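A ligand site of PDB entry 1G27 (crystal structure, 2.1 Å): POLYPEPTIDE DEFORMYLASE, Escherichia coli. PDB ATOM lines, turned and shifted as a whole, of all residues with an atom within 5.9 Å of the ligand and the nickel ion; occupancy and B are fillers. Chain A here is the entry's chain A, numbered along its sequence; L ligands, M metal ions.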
ATOM      1  N   GLU A  41      13.090  12.318   6.264  1.00  0.00           N
ATOM      2  CA  GLU A  41      13.154  13.147   5.040  1.00  0.00           C
ATOM      3  C   GLU A  41      11.817  13.718   4.622  1.00  0.00           C
ATOM      4  O   GLU A  41      11.765  14.558   3.728  1.00  0.00           O
ATOM      5  CB  GLU A  41      13.741  12.333   3.929  1.00  0.00           C
ATOM      6  CG  GLU A  41      15.202  12.179   4.070  1.00  0.00           C
ATOM      7  CD  GLU A  41      15.804  13.408   4.713  1.00  0.00           C
ATOM      8  OE1 GLU A  41      16.636  13.260   5.627  1.00  0.00           O
ATOM      9  OE2 GLU A  41      15.404  14.540   4.337  1.00  0.00           O
ATOM     10  N   GLU A  42      10.745  13.271   5.252  1.00  0.00           N
ATOM     11  CA  GLU A  42       9.396  13.759   4.941  1.00  0.00           C
ATOM     12  C   GLU A  42       8.906  13.371   3.535  1.00  0.00           C
ATOM     13  O   GLU A  42       8.238  14.159   2.848  1.00  0.00           O
ATOM     14  CB  GLU A  42       9.313  15.281   5.133  1.00  0.00           C
ATOM     15  CG  GLU A  42       9.283  15.718   6.583  1.00  0.00           C
ATOM     16  CD  GLU A  42       9.278  17.246   6.744  1.00  0.00           C
ATOM     17  OE1 GLU A  42      10.098  17.930   6.084  1.00  0.00           O
ATOM     18  OE2 GLU A  42       8.454  17.747   7.552  1.00  0.00           O
ATOM     19  N   GLY A  43       9.246  12.148   3.108  1.00  0.00           N
ATOM     20  CA  GLY A  43       8.822  11.652   1.810  1.00  0.00           C
ATOM     21  C   GLY A  43       7.664  10.702   2.033  1.00  0.00           C
ATOM     22  O   GLY A  43       7.384  10.315   3.168  1.00  0.00           O
ATOM     23  N   ILE A  44       6.992  10.312   0.961  1.00  0.00           N
ATOM     24  CA  ILE A  44       5.853   9.392   1.081  1.00  0.00           C
ATOM     25  C   ILE A  44       6.261   8.030   0.564  1.00  0.00           C
ATOM     26  O   ILE A  44       5.485   7.064   0.629  1.00  0.00           O
ATOM     27  CB  ILE A  44       4.644   9.890   0.309  1.00  0.00           C
ATOM     28  CG1 ILE A  44       5.033  10.149  -1.141  1.00  0.00           C
ATOM     29  CG2 ILE A  44       4.121  11.184   0.947  1.00  0.00           C
ATOM     30  CD1 ILE A  44       3.877  10.572  -2.028  1.00  0.00           C
ATOM     31  N   GLY A  45       7.500   7.940   0.091  1.00  0.00           N
ATOM     32  CA  GLY A  45       8.044   6.682  -0.407  1.00  0.00           C
ATOM     33  C   GLY A  45       9.574   6.699  -0.459  1.00  0.00           C
ATOM     34  O   GLY A  45      10.193   7.772  -0.437  1.00  0.00           O
ATOM     35  N   LEU A  46      10.169   5.516  -0.536  1.00  0.00           N
ATOM     36  CA  LEU A  46      11.612   5.380  -0.650  1.00  0.00           C
ATOM     37  C   LEU A  46      11.997   4.038  -1.243  1.00  0.00           C
ATOM     38  O   LEU A  46      11.524   2.990  -0.805  1.00  0.00           O
ATOM     39  CB  LEU A  46      12.287   5.551   0.735  1.00  0.00           C
ATOM     40  CG  LEU A  46      13.807   5.902   0.786  1.00  0.00           C
ATOM     41  CD1 LEU A  46      14.056   7.316   0.322  1.00  0.00           C
ATOM     42  CD2 LEU A  46      14.400   5.692   2.171  1.00  0.00           C
ATOM     43  N   ALA A  47      12.937   4.085  -2.181  1.00  0.00           N
ATOM     44  CA  ALA A  47      13.485   2.890  -2.832  1.00  0.00           C
ATOM     45  C   ALA A  47      14.924   2.672  -2.327  1.00  0.00           C
ATOM     46  O   ALA A  47      15.683   3.606  -2.207  1.00  0.00           O
ATOM     47  CB  ALA A  47      13.499   3.091  -4.378  1.00  0.00           C
ATOM     48  N   GLN A  50      17.979   4.619  -3.560  1.00  0.00           N
ATOM     49  CA  GLN A  50      18.246   5.978  -3.089  1.00  0.00           C
ATOM     50  C   GLN A  50      19.218   6.091  -1.895  1.00  0.00           C
ATOM     51  O   GLN A  50      19.760   7.154  -1.620  1.00  0.00           O
ATOM     52  CB  GLN A  50      16.958   6.678  -2.767  1.00  0.00           C
ATOM     53  CG  GLN A  50      16.191   7.154  -3.954  1.00  0.00           C
ATOM     54  CD  GLN A  50      14.858   7.685  -3.530  1.00  0.00           C
ATOM     55  OE1 GLN A  50      14.032   6.934  -3.016  1.00  0.00           O
ATOM     56  NE2 GLN A  50      14.678   9.011  -3.648  1.00  0.00           N
ATOM     57  N   ILE A  86       0.840  14.030 -11.691  1.00  0.00           N
ATOM     58  CA  ILE A  86       0.826  15.134 -10.742  1.00  0.00           C
ATOM     59  C   ILE A  86       2.208  15.765 -10.790  1.00  0.00           C
ATOM     60  O   ILE A  86       3.073  15.290 -11.526  1.00  0.00           O
ATOM     61  CB  ILE A  86       0.524  14.677  -9.289  1.00  0.00           C
ATOM     62  CG1 ILE A  86       1.428  13.534  -8.871  1.00  0.00           C
ATOM     63  CG2 ILE A  86      -0.876  14.206  -9.154  1.00  0.00           C
ATOM     64  CD1 ILE A  86       1.342  13.227  -7.358  1.00  0.00           C
ATOM     65  N   GLU A  87       2.427  16.812 -10.019  1.00  0.00           N
ATOM     66  CA  GLU A  87       3.764  17.418  -9.932  1.00  0.00           C
ATOM     67  C   GLU A  87       4.538  16.612  -8.898  1.00  0.00           C
ATOM     68  O   GLU A  87       4.327  16.756  -7.705  1.00  0.00           O
ATOM     69  CB  GLU A  87       3.674  18.869  -9.518  1.00  0.00           C
ATOM     70  CG  GLU A  87       2.757  19.677 -10.373  1.00  0.00           C
ATOM     71  CD  GLU A  87       3.392  20.928 -10.896  1.00  0.00           C
ATOM     72  OE1 GLU A  87       4.597  21.147 -10.626  1.00  0.00           O
ATOM     73  OE2 GLU A  87       2.689  21.710 -11.577  1.00  0.00           O
ATOM     74  N   GLU A  88       5.355  15.706  -9.360  1.00  0.00           N
ATOM     75  CA  GLU A  88       6.073  14.858  -8.458  1.00  0.00           C
ATOM     76  C   GLU A  88       7.381  15.518  -8.043  1.00  0.00           C
ATOM     77  O   GLU A  88       7.960  16.328  -8.768  1.00  0.00           O
ATOM     78  CB  GLU A  88       6.402  13.523  -9.116  1.00  0.00           C
ATOM     79  CG  GLU A  88       5.243  12.786  -9.653  1.00  0.00           C
ATOM     80  CD  GLU A  88       5.633  11.376 -10.109  1.00  0.00           C
ATOM     81  OE1 GLU A  88       4.876  10.765 -10.878  1.00  0.00           O
ATOM     82  OE2 GLU A  88       6.708  10.896  -9.698  1.00  0.00           O
ATOM     83  N   GLY A  89       7.880  15.104  -6.906  1.00  0.00           N
ATOM     84  CA  GLY A  89       9.145  15.578  -6.407  1.00  0.00           C
ATOM     85  C   GLY A  89       9.914  14.331  -6.008  1.00  0.00           C
ATOM     86  O   GLY A  89       9.322  13.236  -5.907  1.00  0.00           O
ATOM     87  N   CYS A  90      11.222  14.480  -5.782  1.00  0.00           N
ATOM     88  CA  CYS A  90      12.066  13.346  -5.421  1.00  0.00           C
ATOM     89  C   CYS A  90      13.070  13.730  -4.339  1.00  0.00           C
ATOM     90  O   CYS A  90      13.646  14.810  -4.386  1.00  0.00           O
ATOM     91  CB  CYS A  90      12.828  12.865  -6.658  1.00  0.00           C
ATOM     92  SG  CYS A  90      13.532  11.222  -6.454  1.00  0.00           S
ATOM     93  N   LEU A  91      13.298  12.836  -3.376  1.00  0.00           N
ATOM     94  CA  LEU A  91      14.285  13.094  -2.327  1.00  0.00           C
ATOM     95  C   LEU A  91      15.726  13.185  -2.906  1.00  0.00           C
ATOM     96  O   LEU A  91      16.613  13.777  -2.296  1.00  0.00           O
ATOM     97  CB  LEU A  91      14.208  12.024  -1.266  1.00  0.00           C
ATOM     98  CG  LEU A  91      12.927  12.039  -0.449  1.00  0.00           C
ATOM     99  CD1 LEU A  91      12.985  10.978   0.610  1.00  0.00           C
ATOM    100  CD2 LEU A  91      12.722  13.389   0.199  1.00  0.00           C
ATOM    101  N   SER A  92      15.918  12.620  -4.101  1.00  0.00           N
ATOM    102  CA  SER A  92      17.190  12.610  -4.786  1.00  0.00           C
ATOM    103  C   SER A  92      17.395  13.795  -5.708  1.00  0.00           C
ATOM    104  O   SER A  92      18.480  14.002  -6.257  1.00  0.00           O
ATOM    105  CB  SER A  92      17.365  11.308  -5.519  1.00  0.00           C
ATOM    106  OG  SER A  92      17.296  10.220  -4.599  1.00  0.00           O
ATOM    107  N   GLN A  96      12.915  20.091  -6.576  1.00  0.00           N
ATOM    108  CA  GLN A  96      12.411  20.205  -7.949  1.00  0.00           C
ATOM    109  C   GLN A  96      11.147  19.361  -8.073  1.00  0.00           C
ATOM    110  O   GLN A  96      11.085  18.240  -7.557  1.00  0.00           O
ATOM    111  CB  GLN A  96      13.457  19.733  -8.962  1.00  0.00           C
ATOM    112  CG  GLN A  96      14.771  20.535  -8.951  1.00  0.00           C
ATOM    113  CD  GLN A  96      14.552  22.041  -8.975  1.00  0.00           C
ATOM    114  OE1 GLN A  96      14.047  22.601  -9.957  1.00  0.00           O
ATOM    115  NE2 GLN A  96      14.906  22.695  -7.881  1.00  0.00           N
ATOM    116  N   ARG A  97      10.134  19.906  -8.724  1.00  0.00           N
ATOM    117  CA  ARG A  97       8.874  19.180  -8.912  1.00  0.00           C
ATOM    118  C   ARG A  97       8.399  19.304 -10.365  1.00  0.00           C
ATOM    119  O   ARG A  97       8.624  20.324 -11.014  1.00  0.00           O
ATOM    120  CB  ARG A  97       7.798  19.717  -7.943  1.00  0.00           C
ATOM    121  CG  ARG A  97       8.025  19.364  -6.453  1.00  0.00           C
ATOM    122  CD  ARG A  97       6.809  18.650  -5.861  1.00  0.00           C
ATOM    123  NE  ARG A  97       6.558  19.109  -4.506  1.00  0.00           N
ATOM    124  CZ  ARG A  97       5.367  19.053  -3.901  1.00  0.00           C
ATOM    125  NH1 ARG A  97       5.233  19.507  -2.658  1.00  0.00           N
ATOM    126  NH2 ARG A  97       4.321  18.497  -4.520  1.00  0.00           N
ATOM    127  N   LEU A 125      -2.927   8.655  -5.663  1.00  0.00           N
ATOM    128  CA  LEU A 125      -1.558   8.890  -5.220  1.00  0.00           C
ATOM    129  C   LEU A 125      -0.765   7.617  -5.022  1.00  0.00           C
ATOM    130  O   LEU A 125       0.378   7.529  -5.429  1.00  0.00           O
ATOM    131  CB  LEU A 125      -1.580   9.685  -3.929  1.00  0.00           C
ATOM    132  CG  LEU A 125      -0.228  10.096  -3.358  1.00  0.00           C
ATOM    133  CD1 LEU A 125       0.513  10.951  -4.380  1.00  0.00           C
ATOM    134  CD2 LEU A 125      -0.458  10.864  -2.039  1.00  0.00           C
ATOM    135  N   ILE A 128       0.740   6.166  -8.416  1.00  0.00           N
ATOM    136  CA  ILE A 128       1.781   7.013  -8.983  1.00  0.00           C
ATOM    137  C   ILE A 128       3.062   6.820  -8.173  1.00  0.00           C
ATOM    138  O   ILE A 128       4.138   6.673  -8.725  1.00  0.00           O
ATOM    139  CB  ILE A 128       1.350   8.493  -8.889  1.00  0.00           C
ATOM    140  CG1 ILE A 128       0.201   8.792  -9.844  1.00  0.00           C
ATOM    141  CG2 ILE A 128       2.497   9.433  -9.161  1.00  0.00           C
ATOM    142  CD1 ILE A 128      -0.317  10.191  -9.681  1.00  0.00           C
ATOM    143  N   CYS A 129       2.917   6.776  -6.851  1.00  0.00           N
ATOM    144  CA  CYS A 129       4.069   6.619  -5.955  1.00  0.00           C
ATOM    145  C   CYS A 129       4.737   5.303  -6.224  1.00  0.00           C
ATOM    146  O   CYS A 129       5.974   5.220  -6.389  1.00  0.00           O
ATOM    147  CB  CYS A 129       3.657   6.723  -4.485  1.00  0.00           C
ATOM    148  SG  CYS A 129       5.009   6.372  -3.274  1.00  0.00           S
ATOM    149  N   HIS A 132       6.741   5.633  -9.243  1.00  0.00           N
ATOM    150  CA  HIS A 132       7.889   6.474  -9.003  1.00  0.00           C
ATOM    151  C   HIS A 132       9.009   5.624  -8.380  1.00  0.00           C
ATOM    152  O   HIS A 132      10.148   5.675  -8.826  1.00  0.00           O
ATOM    153  CB  HIS A 132       7.472   7.566  -8.039  1.00  0.00           C
ATOM    154  CG  HIS A 132       8.516   8.589  -7.774  1.00  0.00           C
ATOM    155  ND1 HIS A 132       8.411   9.886  -8.215  1.00  0.00           N
ATOM    156  CD2 HIS A 132       9.655   8.536  -7.028  1.00  0.00           C
ATOM    157  CE1 HIS A 132       9.446  10.585  -7.789  1.00  0.00           C
ATOM    158  NE2 HIS A 132      10.205   9.797  -7.043  1.00  0.00           N
ATOM    159  N   GLU A 133       8.661   4.810  -7.375  1.00  0.00           N
ATOM    160  CA  GLU A 133       9.623   3.956  -6.669  1.00  0.00           C
ATOM    161  C   GLU A 133      10.203   2.841  -7.533  1.00  0.00           C
ATOM    162  O   GLU A 133      11.395   2.540  -7.467  1.00  0.00           O
ATOM    163  CB  GLU A 133       9.001   3.325  -5.391  1.00  0.00           C
ATOM    164  CG  GLU A 133       8.355   4.329  -4.348  1.00  0.00           C
ATOM    165  CD  GLU A 133       9.148   5.629  -4.180  1.00  0.00           C
ATOM    166  OE1 GLU A 133      10.364   5.630  -4.458  1.00  0.00           O
ATOM    167  OE2 GLU A 133       8.556   6.641  -3.780  1.00  0.00           O
ATOM    168  N   HIS A 136      12.891   3.845  -9.721  1.00  0.00           N
ATOM    169  CA  HIS A 136      14.173   4.021  -9.008  1.00  0.00           C
ATOM    170  C   HIS A 136      14.977   2.751  -9.093  1.00  0.00           C
ATOM    171  O   HIS A 136      16.164   2.791  -9.338  1.00  0.00           O
ATOM    172  CB  HIS A 136      13.953   4.367  -7.481  1.00  0.00           C
ATOM    173  CG  HIS A 136      13.848   5.826  -7.180  1.00  0.00           C
ATOM    174  ND1 HIS A 136      14.793   6.746  -7.585  1.00  0.00           N
ATOM    175  CD2 HIS A 136      12.893   6.533  -6.528  1.00  0.00           C
ATOM    176  CE1 HIS A 136      14.434   7.955  -7.210  1.00  0.00           C
ATOM    177  NE2 HIS A 136      13.277   7.857  -6.564  1.00  0.00           N
HETATM  178  C1  LIG L   1      10.272  10.571  -2.390  1.00  0.00           C
HETATM  179  C2  LIG L   1       9.085  11.153  -3.127  1.00  0.00           C
HETATM  180  C3  LIG L   1       8.350  12.150  -2.278  1.00  0.00           C
HETATM  181  O1  LIG L   1       8.039  11.851  -1.123  1.00  0.00           O
HETATM  182  N1  LIG L   1       7.947  13.278  -2.896  1.00  0.00           N
HETATM  183  C4  LIG L   1       7.104  14.253  -2.268  1.00  0.00           C
HETATM  184  C5  LIG L   1       8.134  10.108  -3.766  1.00  0.00           C
HETATM  185  C6  LIG L   1       7.064  10.813  -4.683  1.00  0.00           C
HETATM  186  C7  LIG L   1       5.872   9.868  -4.941  1.00  0.00           C
HETATM  187  C8  LIG L   1       5.099  10.259  -6.201  1.00  0.00           C
HETATM  188  N2  LIG L   1      11.167   9.891  -3.311  1.00  0.00           N
HETATM  189  C9  LIG L   1      11.035   8.587  -3.519  1.00  0.00           C
HETATM  190  O2  LIG L   1      11.696   8.013  -4.392  1.00  0.00           O
HETATM  191  O3  LIG L   1      12.010  10.483  -4.166  1.00  0.00           O
HETATM  192  C10 LIG L   1       6.010  14.531  -3.282  1.00  0.00           C
HETATM  193  N3  LIG L   1       4.681  14.455  -3.077  1.00  0.00           N
HETATM  194  C11 LIG L   1       3.813  14.751  -4.210  1.00  0.00           C
HETATM  195  C12 LIG L   1       4.114  14.138  -1.784  1.00  0.00           C
HETATM  196  O4  LIG L   1       6.429  14.797  -4.418  1.00  0.00           O
HETATM  197  C13 LIG L   1       7.822  15.518  -1.772  1.00  0.00           C
HETATM  198  C14 LIG L   1       6.780  16.462  -1.135  1.00  0.00           C
HETATM  199  C15 LIG L   1       8.522  16.259  -2.924  1.00  0.00           C
HETATM  200  C16 LIG L   1       8.863  15.131  -0.723  1.00  0.00           C
HETATM  201 NI    NI M   1      12.207   9.566  -5.797  1.00  0.00          NI
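The nickel ion is bound by an oxygen (O3) of the ligand (1.9 Å), an oxygen (O2) of the ligand (2.2 Å), a ring nitrogen (NE2) of His 136 (2.2 Å), the side-chain sulfur (SG) of Cys 90 (2.2 Å) and a ring nitrogen (NE2) of His 132 (2.4 Å). The nickel ion has five donor atoms within binding distance.
O of Glu 42 touches C16 of the ligand, 3.8 Å away. Gly 43 touches the ligand. Gly 45 touches the ligand. Glu 88 touches the ligand. Arg 97 touches the ligand. Cys 129 touches the ligand (CA to C8, 3.8 Å). Hydrophobic or aromatic side chains within 4 Å of the ligand: Ile 44, Leu 91, His 132 and His 136. The nearest printed residue that does not touch the ligand is Ile 128 (4.03 Å).
O2 of the ligand lies close to OE1 of Glu 133, 2.7 Å away. N of Ile 44 lies within hydrogen-bond range of O1 of the ligand (2.8 Å). An oxygen (O3) of the ligand sits close to the backbone NH (N) of Leu 91, 2.8 Å away. O4 of the ligand is in hydrogen-bond range of N of Gly 89, at 2.9 Å. N1 of the ligand is in hydrogen-bond range of O of Gly 89, at 3.3 Å. The side-chain amide oxygen (OE1) of Gln 50 sits close to an oxygen (O2) of the ligand (2.9 Å).
The side-chain amide nitrogen of Gln 50 sits close to a ring nitrogen (NE2) of His 136 (3.4 Å). The side-chain amide nitrogen (NE2) of Gln 50 lies close to the side-chain sulfur (SG) of Cys 90 (3.8 Å). The backbone NH of Ser 92 sits close to the side-chain sulfur of Cys 90 (3.6 Å). A ring nitrogen (ND1) of His 132 lies within hydrogen-bond range of the side-chain carboxylate (OE2) of Glu 88 (2.5 Å). The side-chain sulfur (SG) of Cys 129 is in hydrogen-bond range of the side-chain carboxylate (OE2) of Glu 133 (3.6 Å). The side-chain hydroxyl of Ser 92 lies within hydrogen-bond range of the side-chain amide nitrogen of Gln 50 (3.0 Å). The backbone NH (N) of Ala 47 is in hydrogen-bond range of the side-chain amide oxygen (OE1) of Gln 50 (3.2 Å).
Residues that only touch the nickel ion: Gln 50 (3.3 Å). Of the 23 residues printed, 4 come within 4 Å of the nickel ion. Along chain A the residues within 4 Å of the nickel ion span positions 50 to 136.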
